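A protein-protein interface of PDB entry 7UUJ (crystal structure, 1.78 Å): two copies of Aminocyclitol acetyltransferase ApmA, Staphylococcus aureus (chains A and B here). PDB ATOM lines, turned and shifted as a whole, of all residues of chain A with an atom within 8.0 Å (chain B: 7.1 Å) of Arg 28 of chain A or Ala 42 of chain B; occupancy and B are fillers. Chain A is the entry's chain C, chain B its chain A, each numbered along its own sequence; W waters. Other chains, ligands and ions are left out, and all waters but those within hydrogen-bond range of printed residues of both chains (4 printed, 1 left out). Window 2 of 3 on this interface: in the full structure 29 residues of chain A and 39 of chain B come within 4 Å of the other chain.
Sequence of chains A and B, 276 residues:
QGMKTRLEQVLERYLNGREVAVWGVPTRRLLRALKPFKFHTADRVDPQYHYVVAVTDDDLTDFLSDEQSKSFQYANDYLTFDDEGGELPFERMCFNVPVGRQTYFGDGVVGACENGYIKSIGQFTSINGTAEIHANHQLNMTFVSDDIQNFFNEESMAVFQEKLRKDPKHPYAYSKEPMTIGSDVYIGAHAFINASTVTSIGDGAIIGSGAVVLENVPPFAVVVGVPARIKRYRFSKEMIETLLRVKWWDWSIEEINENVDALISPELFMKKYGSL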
ATOM      1  N   VAL A  25      29.042  11.195  -7.272  1.00  0.00           N
ATOM      2  CA  VAL A  25      28.598  11.790  -6.008  1.00  0.00           C
ATOM      3  C   VAL A  25      27.256  11.163  -5.641  1.00  0.00           C
ATOM      4  O   VAL A  25      26.299  11.220  -6.435  1.00  0.00           O
ATOM      5  CB  VAL A  25      28.513  13.322  -6.095  1.00  0.00           C
ATOM      6  CG1 VAL A  25      27.900  13.921  -4.800  1.00  0.00           C
ATOM      7  CG2 VAL A  25      29.885  13.907  -6.415  1.00  0.00           C
ATOM      8  N   PRO A  26      27.153  10.511  -4.484  1.00  0.00           N
ATOM      9  CA  PRO A  26      25.877   9.882  -4.109  1.00  0.00           C
ATOM     10  C   PRO A  26      24.819  10.920  -3.761  1.00  0.00           C
ATOM     11  O   PRO A  26      25.106  11.959  -3.168  1.00  0.00           O
ATOM     12  CB  PRO A  26      26.248   9.002  -2.908  1.00  0.00           C
ATOM     13  CG  PRO A  26      27.577   9.516  -2.433  1.00  0.00           C
ATOM     14  CD  PRO A  26      28.268  10.105  -3.609  1.00  0.00           C
ATOM     15  N   THR A  27      23.597  10.650  -4.183  1.00  0.00           N
ATOM     16  CA  THR A  27      22.480  11.558  -3.968  1.00  0.00           C
ATOM     17  C   THR A  27      21.537  10.997  -2.916  1.00  0.00           C
ATOM     18  O   THR A  27      21.632   9.832  -2.526  1.00  0.00           O
ATOM     19  CB  THR A  27      21.716  11.789  -5.269  1.00  0.00           C
ATOM     20  OG1 THR A  27      21.125  10.539  -5.665  1.00  0.00           O
ATOM     21  CG2 THR A  27      22.663  12.295  -6.355  1.00  0.00           C
ATOM     22  N   ARG A  28      20.622  11.861  -2.463  1.00  0.00           N
ATOM     23  CA  ARG A  28      19.599  11.411  -1.519  1.00  0.00           C
ATOM     24  C   ARG A  28      18.782  10.266  -2.122  1.00  0.00           C
ATOM     25  O   ARG A  28      18.581   9.229  -1.472  1.00  0.00           O
ATOM     26  CB  ARG A  28      18.699  12.574  -1.103  1.00  0.00           C
ATOM     27  CG  ARG A  28      19.401  13.541  -0.131  1.00  0.00           C
ATOM     28  CD  ARG A  28      18.951  13.326   1.267  1.00  0.00           C
ATOM     29  NE  ARG A  28      19.501  14.296   2.201  1.00  0.00           N
ATOM     30  CZ  ARG A  28      19.159  14.371   3.477  1.00  0.00           C
ATOM     31  NH1 ARG A  28      18.288  13.534   4.002  1.00  0.00           N
ATOM     32  NH2 ARG A  28      19.708  15.306   4.242  1.00  0.00           N
ATOM     33  N   ARG A  29      18.350  10.407  -3.392  1.00  0.00           N
ATOM     34  CA  ARG A  29      17.538   9.353  -3.993  1.00  0.00           C
ATOM     35  C   ARG A  29      18.327   8.049  -4.146  1.00  0.00           C
ATOM     36  O   ARG A  29      17.776   6.957  -3.954  1.00  0.00           O
ATOM     37  CB  ARG A  29      16.995   9.809  -5.342  1.00  0.00           C
ATOM     38  CG  ARG A  29      15.784   9.023  -5.769  1.00  0.00           C
ATOM     39  CD  ARG A  29      15.035   9.715  -6.884  1.00  0.00           C
ATOM     40  NE  ARG A  29      15.854   9.754  -8.092  1.00  0.00           N
ATOM     41  CZ  ARG A  29      15.867   8.811  -9.025  1.00  0.00           C
ATOM     42  NH1 ARG A  29      15.094   7.740  -8.941  1.00  0.00           N
ATOM     43  NH2 ARG A  29      16.680   8.944 -10.071  1.00  0.00           N
ATOM     44  N   LEU A  30      19.603   8.140  -4.524  1.00  0.00           N
ATOM     45  CA  LEU A  30      20.432   6.943  -4.657  1.00  0.00           C
ATOM     46  C   LEU A  30      20.628   6.234  -3.317  1.00  0.00           C
ATOM     47  O   LEU A  30      20.493   5.008  -3.223  1.00  0.00           O
ATOM     48  CB  LEU A  30      21.777   7.329  -5.238  1.00  0.00           C
ATOM     49  CG  LEU A  30      22.745   6.144  -5.326  1.00  0.00           C
ATOM     50  CD1 LEU A  30      22.199   5.089  -6.252  1.00  0.00           C
ATOM     51  CD2 LEU A  30      24.137   6.593  -5.781  1.00  0.00           C
ATOM     52  N   LEU A  31      20.991   6.985  -2.284  1.00  0.00           N
ATOM     53  CA  LEU A  31      21.210   6.378  -0.970  1.00  0.00           C
ATOM     54  C   LEU A  31      19.950   5.675  -0.459  1.00  0.00           C
ATOM     55  O   LEU A  31      20.032   4.605   0.158  1.00  0.00           O
ATOM     56  CB  LEU A  31      21.665   7.447   0.014  1.00  0.00           C
ATOM     57  CG  LEU A  31      23.057   8.019  -0.190  1.00  0.00           C
ATOM     58  CD1 LEU A  31      23.246   9.206   0.739  1.00  0.00           C
ATOM     59  CD2 LEU A  31      24.090   6.954   0.074  1.00  0.00           C
ATOM     60  N   ARG A  32      18.775   6.264  -0.697  1.00  0.00           N
ATOM     61  CA  ARG A  32      17.542   5.591  -0.296  1.00  0.00           C
ATOM     62  C   ARG A  32      17.356   4.279  -1.048  1.00  0.00           C
ATOM     63  O   ARG A  32      16.982   3.259  -0.443  1.00  0.00           O
ATOM     64  CB  ARG A  32      16.329   6.494  -0.508  1.00  0.00           C
ATOM     65  CG  ARG A  32      15.093   5.964   0.279  1.00  0.00           C
ATOM     66  CD  ARG A  32      13.950   6.897   0.292  1.00  0.00           C
ATOM     67  NE  ARG A  32      14.254   8.139   0.987  1.00  0.00           N
ATOM     68  CZ  ARG A  32      13.911   8.416   2.228  1.00  0.00           C
ATOM     69  NH1 ARG A  32      13.283   7.531   2.991  1.00  0.00           N
ATOM     70  NH2 ARG A  32      14.157   9.630   2.710  1.00  0.00           N
ATOM     71  N   ALA A  33      17.604   4.284  -2.363  1.00  0.00           N
ATOM     72  CA  ALA A  33      17.447   3.072  -3.164  1.00  0.00           C
ATOM     73  C   ALA A  33      18.454   1.990  -2.768  1.00  0.00           C
ATOM     74  O   ALA A  33      18.179   0.799  -2.950  1.00  0.00           O
ATOM     75  CB  ALA A  33      17.596   3.398  -4.649  1.00  0.00           C
ATOM     76  N   LEU A  34      19.611   2.383  -2.247  1.00  0.00           N
ATOM     77  CA  LEU A  34      20.676   1.453  -1.870  1.00  0.00           C
ATOM     78  C   LEU A  34      20.555   0.923  -0.449  1.00  0.00           C
ATOM     79  O   LEU A  34      21.331   0.039  -0.072  1.00  0.00           O
ATOM     80  CB  LEU A  34      22.047   2.125  -2.018  1.00  0.00           C
ATOM     81  CG  LEU A  34      22.495   2.302  -3.460  1.00  0.00           C
ATOM     82  CD1 LEU A  34      23.830   3.045  -3.521  1.00  0.00           C
ATOM     83  CD2 LEU A  34      22.563   0.953  -4.207  1.00  0.00           C
ATOM     84  N   VAL A  55      26.407   7.261 -11.101  1.00  0.00           N
ATOM     85  CA  VAL A  55      25.251   8.026 -10.642  1.00  0.00           C
ATOM     86  C   VAL A  55      24.578   8.720 -11.828  1.00  0.00           C
ATOM     87  O   VAL A  55      23.364   8.593 -12.030  1.00  0.00           O
ATOM     88  CB  VAL A  55      25.659   9.019  -9.546  1.00  0.00           C
ATOM     89  CG1 VAL A  55      24.428   9.782  -9.011  1.00  0.00           C
ATOM     90  CG2 VAL A  55      26.356   8.268  -8.421  1.00  0.00           C
ATOM     91  N   PHE A  81      22.418   5.127 -12.452  1.00  0.00           N
ATOM     92  CA  PHE A  81      21.271   5.325 -11.576  1.00  0.00           C
ATOM     93  C   PHE A  81      20.249   6.269 -12.194  1.00  0.00           C
ATOM     94  O   PHE A  81      19.036   6.016 -12.142  1.00  0.00           O
ATOM     95  CB  PHE A  81      21.733   5.882 -10.246  1.00  0.00           C
ATOM     96  CG  PHE A  81      20.613   6.193  -9.326  1.00  0.00           C
ATOM     97  CD1 PHE A  81      19.747   5.195  -8.923  1.00  0.00           C
ATOM     98  CD2 PHE A  81      20.406   7.490  -8.875  1.00  0.00           C
ATOM     99  CE1 PHE A  81      18.697   5.484  -8.059  1.00  0.00           C
ATOM    100  CE2 PHE A  81      19.374   7.774  -8.011  1.00  0.00           C
ATOM    101  CZ  PHE A  81      18.510   6.774  -7.622  1.00  0.00           C
ATOM    102  N   VAL B  20      16.931  26.739   7.942  1.00  0.00           N
ATOM    103  CA  VAL B  20      16.774  26.031   6.674  1.00  0.00           C
ATOM    104  C   VAL B  20      17.424  24.665   6.797  1.00  0.00           C
ATOM    105  O   VAL B  20      18.594  24.559   7.171  1.00  0.00           O
ATOM    106  CB  VAL B  20      17.393  26.825   5.515  1.00  0.00           C
ATOM    107  CG1 VAL B  20      17.490  25.946   4.250  1.00  0.00           C
ATOM    108  CG2 VAL B  20      16.563  28.124   5.264  1.00  0.00           C
ATOM    109  N   ALA B  21      16.682  23.617   6.466  1.00  0.00           N
ATOM    110  CA  ALA B  21      17.234  22.265   6.500  1.00  0.00           C
ATOM    111  C   ALA B  21      17.440  21.833   5.053  1.00  0.00           C
ATOM    112  O   ALA B  21      16.467  21.648   4.311  1.00  0.00           O
ATOM    113  CB  ALA B  21      16.309  21.312   7.240  1.00  0.00           C
ATOM    114  N   VAL B  22      18.703  21.712   4.651  1.00  0.00           N
ATOM    115  CA  VAL B  22      19.046  21.445   3.256  1.00  0.00           C
ATOM    116  C   VAL B  22      18.960  19.949   3.013  1.00  0.00           C
ATOM    117  O   VAL B  22      19.632  19.154   3.679  1.00  0.00           O
ATOM    118  CB  VAL B  22      20.443  21.982   2.926  1.00  0.00           C
ATOM    119  CG1 VAL B  22      20.870  21.618   1.476  1.00  0.00           C
ATOM    120  CG2 VAL B  22      20.426  23.483   3.104  1.00  0.00           C
ATOM    121  N   TRP B  23      18.086  19.564   2.100  1.00  0.00           N
ATOM    122  CA  TRP B  23      17.847  18.167   1.757  1.00  0.00           C
ATOM    123  C   TRP B  23      18.528  17.909   0.412  1.00  0.00           C
ATOM    124  O   TRP B  23      17.942  18.187  -0.632  1.00  0.00           O
ATOM    125  CB  TRP B  23      16.311  17.933   1.697  1.00  0.00           C
ATOM    126  CG  TRP B  23      15.877  16.515   1.764  1.00  0.00           C
ATOM    127  CD1 TRP B  23      15.885  15.597   0.742  1.00  0.00           C
ATOM    128  CD2 TRP B  23      15.326  15.844   2.904  1.00  0.00           C
ATOM    129  NE1 TRP B  23      15.408  14.381   1.202  1.00  0.00           N
ATOM    130  CE2 TRP B  23      15.058  14.517   2.521  1.00  0.00           C
ATOM    131  CE3 TRP B  23      15.064  16.235   4.230  1.00  0.00           C
ATOM    132  CZ2 TRP B  23      14.514  13.584   3.403  1.00  0.00           C
ATOM    133  CZ3 TRP B  23      14.531  15.316   5.096  1.00  0.00           C
ATOM    134  CH2 TRP B  23      14.270  13.993   4.687  1.00  0.00           C
ATOM    135  N   GLY B  24      19.762  17.387   0.438  1.00  0.00           N
ATOM    136  CA  GLY B  24      20.524  17.161  -0.771  1.00  0.00           C
ATOM    137  C   GLY B  24      21.891  17.812  -0.705  1.00  0.00           C
ATOM    138  O   GLY B  24      22.247  18.493   0.254  1.00  0.00           O
ATOM    139  N   VAL B  25      22.662  17.612  -1.774  1.00  0.00           N
ATOM    140  CA  VAL B  25      24.027  18.133  -1.838  1.00  0.00           C
ATOM    141  C   VAL B  25      23.991  19.636  -2.099  1.00  0.00           C
ATOM    142  O   VAL B  25      23.397  20.088  -3.090  1.00  0.00           O
ATOM    143  CB  VAL B  25      24.848  17.396  -2.905  1.00  0.00           C
ATOM    144  CG1 VAL B  25      26.297  17.906  -2.922  1.00  0.00           C
ATOM    145  CG2 VAL B  25      24.819  15.885  -2.655  1.00  0.00           C
ATOM    146  N   HIS B  40      21.363  24.200   7.938  1.00  0.00           N
ATOM    147  CA  HIS B  40      22.151  23.012   8.249  1.00  0.00           C
ATOM    148  C   HIS B  40      21.686  21.886   7.340  1.00  0.00           C
ATOM    149  O   HIS B  40      20.569  21.919   6.821  1.00  0.00           O
ATOM    150  CB  HIS B  40      22.002  22.620   9.722  1.00  0.00           C
ATOM    151  CG  HIS B  40      23.063  21.679  10.201  1.00  0.00           C
ATOM    152  ND1 HIS B  40      22.877  20.314  10.274  1.00  0.00           N
ATOM    153  CD2 HIS B  40      24.331  21.910  10.621  1.00  0.00           C
ATOM    154  CE1 HIS B  40      23.982  19.746  10.731  1.00  0.00           C
ATOM    155  NE2 HIS B  40      24.879  20.692  10.952  1.00  0.00           N
ATOM    156  N   THR B  41      22.544  20.877   7.151  1.00  0.00           N
ATOM    157  CA  THR B  41      22.099  19.727   6.373  1.00  0.00           C
ATOM    158  C   THR B  41      20.984  19.016   7.128  1.00  0.00           C
ATOM    159  O   THR B  41      21.013  18.905   8.363  1.00  0.00           O
ATOM    160  CB  THR B  41      23.256  18.756   6.105  1.00  0.00           C
ATOM    161  OG1 THR B  41      23.814  18.364   7.347  1.00  0.00           O
ATOM    162  CG2 THR B  41      24.326  19.449   5.322  1.00  0.00           C
ATOM    163  N   ALA B  42      19.976  18.554   6.390  1.00  0.00           N
ATOM    164  CA  ALA B  42      18.782  18.007   7.022  1.00  0.00           C
ATOM    165  C   ALA B  42      19.032  16.621   7.603  1.00  0.00           C
ATOM    166  O   ALA B  42      19.627  15.754   6.947  1.00  0.00           O
ATOM    167  CB  ALA B  42      17.632  17.946   6.020  1.00  0.00           C
ATOM    168  N   ASP B  43      18.592  16.409   8.842  1.00  0.00           N
ATOM    169  CA  ASP B  43      18.555  15.052   9.374  1.00  0.00           C
ATOM    170  C   ASP B  43      17.112  14.793   9.773  1.00  0.00           C
ATOM    171  O   ASP B  43      16.300  14.396   8.930  1.00  0.00           O
ATOM    172  CB  ASP B  43      19.546  14.835  10.521  1.00  0.00           C
ATOM    173  CG  ASP B  43      19.638  16.022  11.485  1.00  0.00           C
ATOM    174  OD1 ASP B  43      18.672  16.269  12.258  1.00  0.00           O
ATOM    175  OD2 ASP B  43      20.704  16.686  11.493  1.00  0.00           O
ATOM    176  N   ARG B  44      16.764  15.047  11.023  1.00  0.00           N
ATOM    177  CA  ARG B  44      15.370  15.045  11.432  1.00  0.00           C
ATOM    178  C   ARG B  44      14.806  16.451  11.275  1.00  0.00           C
ATOM    179  O   ARG B  44      15.463  17.432  11.643  1.00  0.00           O
ATOM    180  CB  ARG B  44      15.248  14.570  12.875  1.00  0.00           C
ATOM    181  CG  ARG B  44      15.878  13.215  13.148  1.00  0.00           C
ATOM    182  CD  ARG B  44      14.826  12.095  13.260  1.00  0.00           C
ATOM    183  NE  ARG B  44      15.370  10.936  13.959  1.00  0.00           N
ATOM    184  CZ  ARG B  44      14.711   9.807  14.206  1.00  0.00           C
ATOM    185  NH1 ARG B  44      13.462   9.626  13.804  1.00  0.00           N
ATOM    186  NH2 ARG B  44      15.319   8.840  14.877  1.00  0.00           N
ATOM    187  N   VAL B  45      13.603  16.556  10.713  1.00  0.00           N
ATOM    188  CA  VAL B  45      13.021  17.860  10.428  1.00  0.00           C
ATOM    189  C   VAL B  45      11.606  17.916  11.001  1.00  0.00           C
ATOM    190  O   VAL B  45      10.931  16.894  11.154  1.00  0.00           O
ATOM    191  CB  VAL B  45      13.016  18.193   8.908  1.00  0.00           C
ATOM    192  CG1 VAL B  45      14.470  18.207   8.330  1.00  0.00           C
ATOM    193  CG2 VAL B  45      12.122  17.229   8.113  1.00  0.00           C
ATOM    194  N   VAL B  52      12.354  23.187   4.837  1.00  0.00           N
ATOM    195  CA  VAL B  52      13.142  22.231   4.057  1.00  0.00           C
ATOM    196  C   VAL B  52      13.410  22.772   2.656  1.00  0.00           C
ATOM    197  O   VAL B  52      12.489  23.184   1.933  1.00  0.00           O
ATOM    198  CB  VAL B  52      12.464  20.849   4.001  1.00  0.00           C
ATOM    199  CG1 VAL B  52      13.161  19.940   2.951  1.00  0.00           C
ATOM    200  CG2 VAL B  52      12.539  20.196   5.371  1.00  0.00           C
ATOM    201  N   VAL B  53      14.674  22.743   2.251  1.00  0.00           N
ATOM    202  CA  VAL B  53      15.063  23.131   0.886  1.00  0.00           C
ATOM    203  C   VAL B  53      15.631  21.887   0.209  1.00  0.00           C
ATOM    204  O   VAL B  53      16.712  21.408   0.560  1.00  0.00           O
ATOM    205  CB  VAL B  53      16.069  24.286   0.861  1.00  0.00           C
ATOM    206  CG1 VAL B  53      16.586  24.537  -0.616  1.00  0.00           C
ATOM    207  CG2 VAL B  53      15.398  25.568   1.401  1.00  0.00           C
ATOM    208  N   ASP B  58      15.125  15.805  -7.928  1.00  0.00           N
ATOM    209  CA  ASP B  58      15.256  14.466  -7.356  1.00  0.00           C
ATOM    210  C   ASP B  58      15.299  14.496  -5.836  1.00  0.00           C
ATOM    211  O   ASP B  58      14.769  13.588  -5.178  1.00  0.00           O
ATOM    212  CB  ASP B  58      16.500  13.792  -7.891  1.00  0.00           C
ATOM    213  CG  ASP B  58      16.194  12.843  -9.015  1.00  0.00           C
ATOM    214  OD1 ASP B  58      15.315  13.165  -9.848  1.00  0.00           O
ATOM    215  OD2 ASP B  58      16.834  11.773  -9.060  1.00  0.00           O
ATOM    216  N   ASP B  59      15.966  15.496  -5.254  1.00  0.00           N
ATOM    217  CA  ASP B  59      15.947  15.644  -3.799  1.00  0.00           C
ATOM    218  C   ASP B  59      14.524  15.824  -3.290  1.00  0.00           C
ATOM    219  O   ASP B  59      14.161  15.309  -2.225  1.00  0.00           O
ATOM    220  CB  ASP B  59      16.797  16.847  -3.364  1.00  0.00           C
ATOM    221  CG  ASP B  59      18.299  16.635  -3.582  1.00  0.00           C
ATOM    222  OD1 ASP B  59      18.792  15.498  -3.398  1.00  0.00           O
ATOM    223  OD2 ASP B  59      18.991  17.621  -3.926  1.00  0.00           O
ATOM    224  N   LEU B  60      13.721  16.609  -4.007  1.00  0.00           N
ATOM    225  CA  LEU B  60      12.345  16.836  -3.591  1.00  0.00           C
ATOM    226  C   LEU B  60      11.540  15.545  -3.637  1.00  0.00           C
ATOM    227  O   LEU B  60      10.782  15.245  -2.709  1.00  0.00           O
ATOM    228  CB  LEU B  60      11.692  17.899  -4.474  1.00  0.00           C
ATOM    229  CG  LEU B  60      10.240  18.181  -4.038  1.00  0.00           C
ATOM    230  CD1 LEU B  60      10.214  18.944  -2.720  1.00  0.00           C
ATOM    231  CD2 LEU B  60       9.472  18.924  -5.095  1.00  0.00           C
ATOM    232  N   ASP B  62      12.664  12.673  -3.158  1.00  0.00           N
ATOM    233  CA  ASP B  62      13.049  11.871  -2.010  1.00  0.00           C
ATOM    234  C   ASP B  62      12.462  12.428  -0.720  1.00  0.00           C
ATOM    235  O   ASP B  62      12.090  11.665   0.176  1.00  0.00           O
ATOM    236  CB  ASP B  62      14.571  11.780  -1.901  1.00  0.00           C
ATOM    237  CG  ASP B  62      15.011  10.991  -0.701  1.00  0.00           C
ATOM    238  OD1 ASP B  62      15.006   9.738  -0.768  1.00  0.00           O
ATOM    239  OD2 ASP B  62      15.322  11.621   0.328  1.00  0.00           O
ATOM    240  N   PHE B  63      12.403  13.754  -0.598  1.00  0.00           N
ATOM    241  CA  PHE B  63      11.781  14.371   0.567  1.00  0.00           C
ATOM    242  C   PHE B  63      10.299  14.026   0.644  1.00  0.00           C
ATOM    243  O   PHE B  63       9.798  13.619   1.693  1.00  0.00           O
ATOM    244  CB  PHE B  63      11.964  15.892   0.521  1.00  0.00           C
ATOM    245  CG  PHE B  63      11.278  16.610   1.668  1.00  0.00           C
ATOM    246  CD1 PHE B  63      11.592  16.271   2.996  1.00  0.00           C
ATOM    247  CD2 PHE B  63      10.338  17.613   1.428  1.00  0.00           C
ATOM    248  CE1 PHE B  63      10.942  16.928   4.079  1.00  0.00           C
ATOM    249  CE2 PHE B  63       9.738  18.289   2.479  1.00  0.00           C
ATOM    250  CZ  PHE B  63      10.041  17.947   3.797  1.00  0.00           C
ATOM    251  N   ASP B  66       9.340  10.772   1.892  1.00  0.00           N
ATOM    252  CA  ASP B  66       9.779  10.481   3.242  1.00  0.00           C
ATOM    253  C   ASP B  66       8.653  10.777   4.223  1.00  0.00           C
ATOM    254  O   ASP B  66       7.894  11.734   4.043  1.00  0.00           O
ATOM    255  CB  ASP B  66      10.998  11.330   3.592  1.00  0.00           C
ATOM    256  CG  ASP B  66      11.684  10.873   4.833  1.00  0.00           C
ATOM    257  OD1 ASP B  66      11.095  10.994   5.961  1.00  0.00           O
ATOM    258  OD2 ASP B  66      12.816  10.373   4.693  1.00  0.00           O
ATOM    259  N   GLN B  68       8.813  12.066   7.046  1.00  0.00           N
ATOM    260  CA  GLN B  68       8.955  13.378   7.664  1.00  0.00           C
ATOM    261  C   GLN B  68       8.279  14.520   6.899  1.00  0.00           C
ATOM    262  O   GLN B  68       8.057  15.576   7.491  1.00  0.00           O
ATOM    263  CB  GLN B  68      10.429  13.718   7.830  1.00  0.00           C
ATOM    264  CG  GLN B  68      11.164  12.719   8.719  1.00  0.00           C
ATOM    265  CD  GLN B  68      12.505  13.237   9.176  1.00  0.00           C
ATOM    266  OE1 GLN B  68      12.590  13.984  10.156  1.00  0.00           O
ATOM    267  NE2 GLN B  68      13.559  12.882   8.447  1.00  0.00           N
HETATM  268  O   HOH W   1      17.264  11.179   2.430  1.00  0.00           O
HETATM  269  O   HOH W   2      21.231  14.669  -3.010  1.00  0.00           O
HETATM  270  O   HOH W   3      17.423  13.358   6.582  1.00  0.00           O
HETATM  271  O   HOH W   4      18.393  13.017  -4.659  1.00  0.00           O
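Val 25 of chain B touches Pro 26 of chain A. Val 22 of chain B touches Arg 28 of chain A. CE2 of Trp 23 of chain B touches NH1 of Arg 28 of chain A, 3.7 Å away. Arg 28 of chain A touches Gly 24 of chain B. Arg 28 of chain A touches Asp 59 of chain B (CB to OD1, 3.7 Å). Asp 62 of chain B touches Arg 28 of chain A (OD1 to O, 3.7 Å).
Of the 21 printed residues of chain B, 9 touch a printed residue of chain A. Printed residues of chain B that touch a printed residue of chain A: Val 22, Trp 23, Gly 24, Val 25, Ala 42, Asp 58, Asp 59, Asp 62 and Asp 66. Hydrophobic or aromatic side chains of chain B within 4 Å of the printed part of chain A: Trp 23, Val 25 and Ala 42. Among the printed residues, Asp or Glu carboxylates within 4 Å of a Lys or Arg side-chain nitrogen of the other chain: Arg 29 of chain A with Asp 58 of chain B (2.4 Å), Arg 32 of chain A with Asp 62 of chain B (2.5 Å) and Arg 32 of chain A with Asp 66 of chain B (2.5 Å).
Of chain B, only Val 22, Trp 23, Gly 24, Ala 42, Asp 59 and Asp 62 come within 4 Å of Arg 28 of chain A. Ala 42 of chain B touches just one residue of chain A: Arg 28 (2.7 Å). Of the printed residues of chain B, Arg 29 of chain A touches Asp 58. Of the printed residues of chain A, Gly 24 of chain B touches Arg 28 (3.6 Å). Printed residues of chain A within 4 Å of Val 25 of chain B: Pro 26 (3.97 Å). Of the printed residues of chain A, Asp 62 of chain B touches Arg 28 (3.7 Å) and Arg 32 (2.5 Å). Asp 43 of chain B touches none of the printed residues of chain A. Phe 63 of chain B touches none of the printed residues of chain A. The nearest printed residue of chain B that does not touch Arg 28 of chain A is Asp 43 of chain B (4.9 Å). The nearest printed residue of chain A that does not touch Ala 42 of chain B is Arg 32 of chain A (9.2 Å).
Water W2 lies within hydrogen-bond range of OD1 of Asp 59 of chain B (2.6 Å), N of Arg 28 of chain A (2.9 Å) and N of Val 25 of chain B (3.5 Å). Water W3 lies within hydrogen-bond range of NH1 of Arg 28 of chain A (2.7 Å), O of Asp 43 of chain B (2.8 Å) and O of Ala 42 of chain B (3.3 Å). Water W4 lies within hydrogen-bond range of OD1 of Asp 59 of chain B (2.8 Å), N of Arg 29 of chain A (2.9 Å) and N of Arg 28 of chain A (3.3 Å). Water W1 lies within hydrogen-bond range of the side-chain carboxylate (OD2) of Asp 62 of chain B (2.9 Å), the guanidinium group (NH1) of Arg 28 of chain A (3.0 Å) and the guanidinium group (NH2) of Arg 32 of chain A (3.5 Å).
The backbone carbonyl oxygen (O) of His 40 of chain B lies within hydrogen-bond range of the backbone NH (N) of Val 22 of chain B (2.9 Å). The backbone carbonyl oxygen of Val 22 of chain B lies within hydrogen-bond range of the backbone NH of Ala 42 of chain B (2.8 Å). The backbone NH of Trp 23 of chain B lies within hydrogen-bond range of the backbone carbonyl oxygen of Val 53 of chain B (2.8 Å). The indole nitrogen of Trp 23 of chain B sits at hydrogen-bond distance from the side-chain carboxylate of Asp 62 of chain B, 2.9 Å away. OD1 of Asp 66 of chain B sits at hydrogen-bond distance from N of Gln 68 of chain B, 2.7 Å away.
Position printed for both chains: 25.
The backbone carbonyl oxygen of Ala 42 of chain B is in hydrogen-bond range of the guanidinium group of Arg 28 of chain A, at 2.7 Å. NE of Arg 29 of chain A is in salt-bridge range of OD2 of Asp 58 of chain B (2.4 Å). The side-chain carboxylate (OD1) of Asp 62 of chain B is in salt-bridge range of the guanidinium group (NE) of Arg 32 of chain A, at 2.5 Å. OD2 of Asp 66 of chain B lies within salt-bridge range of NH2 of Arg 32 of chain A (2.5 Å).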
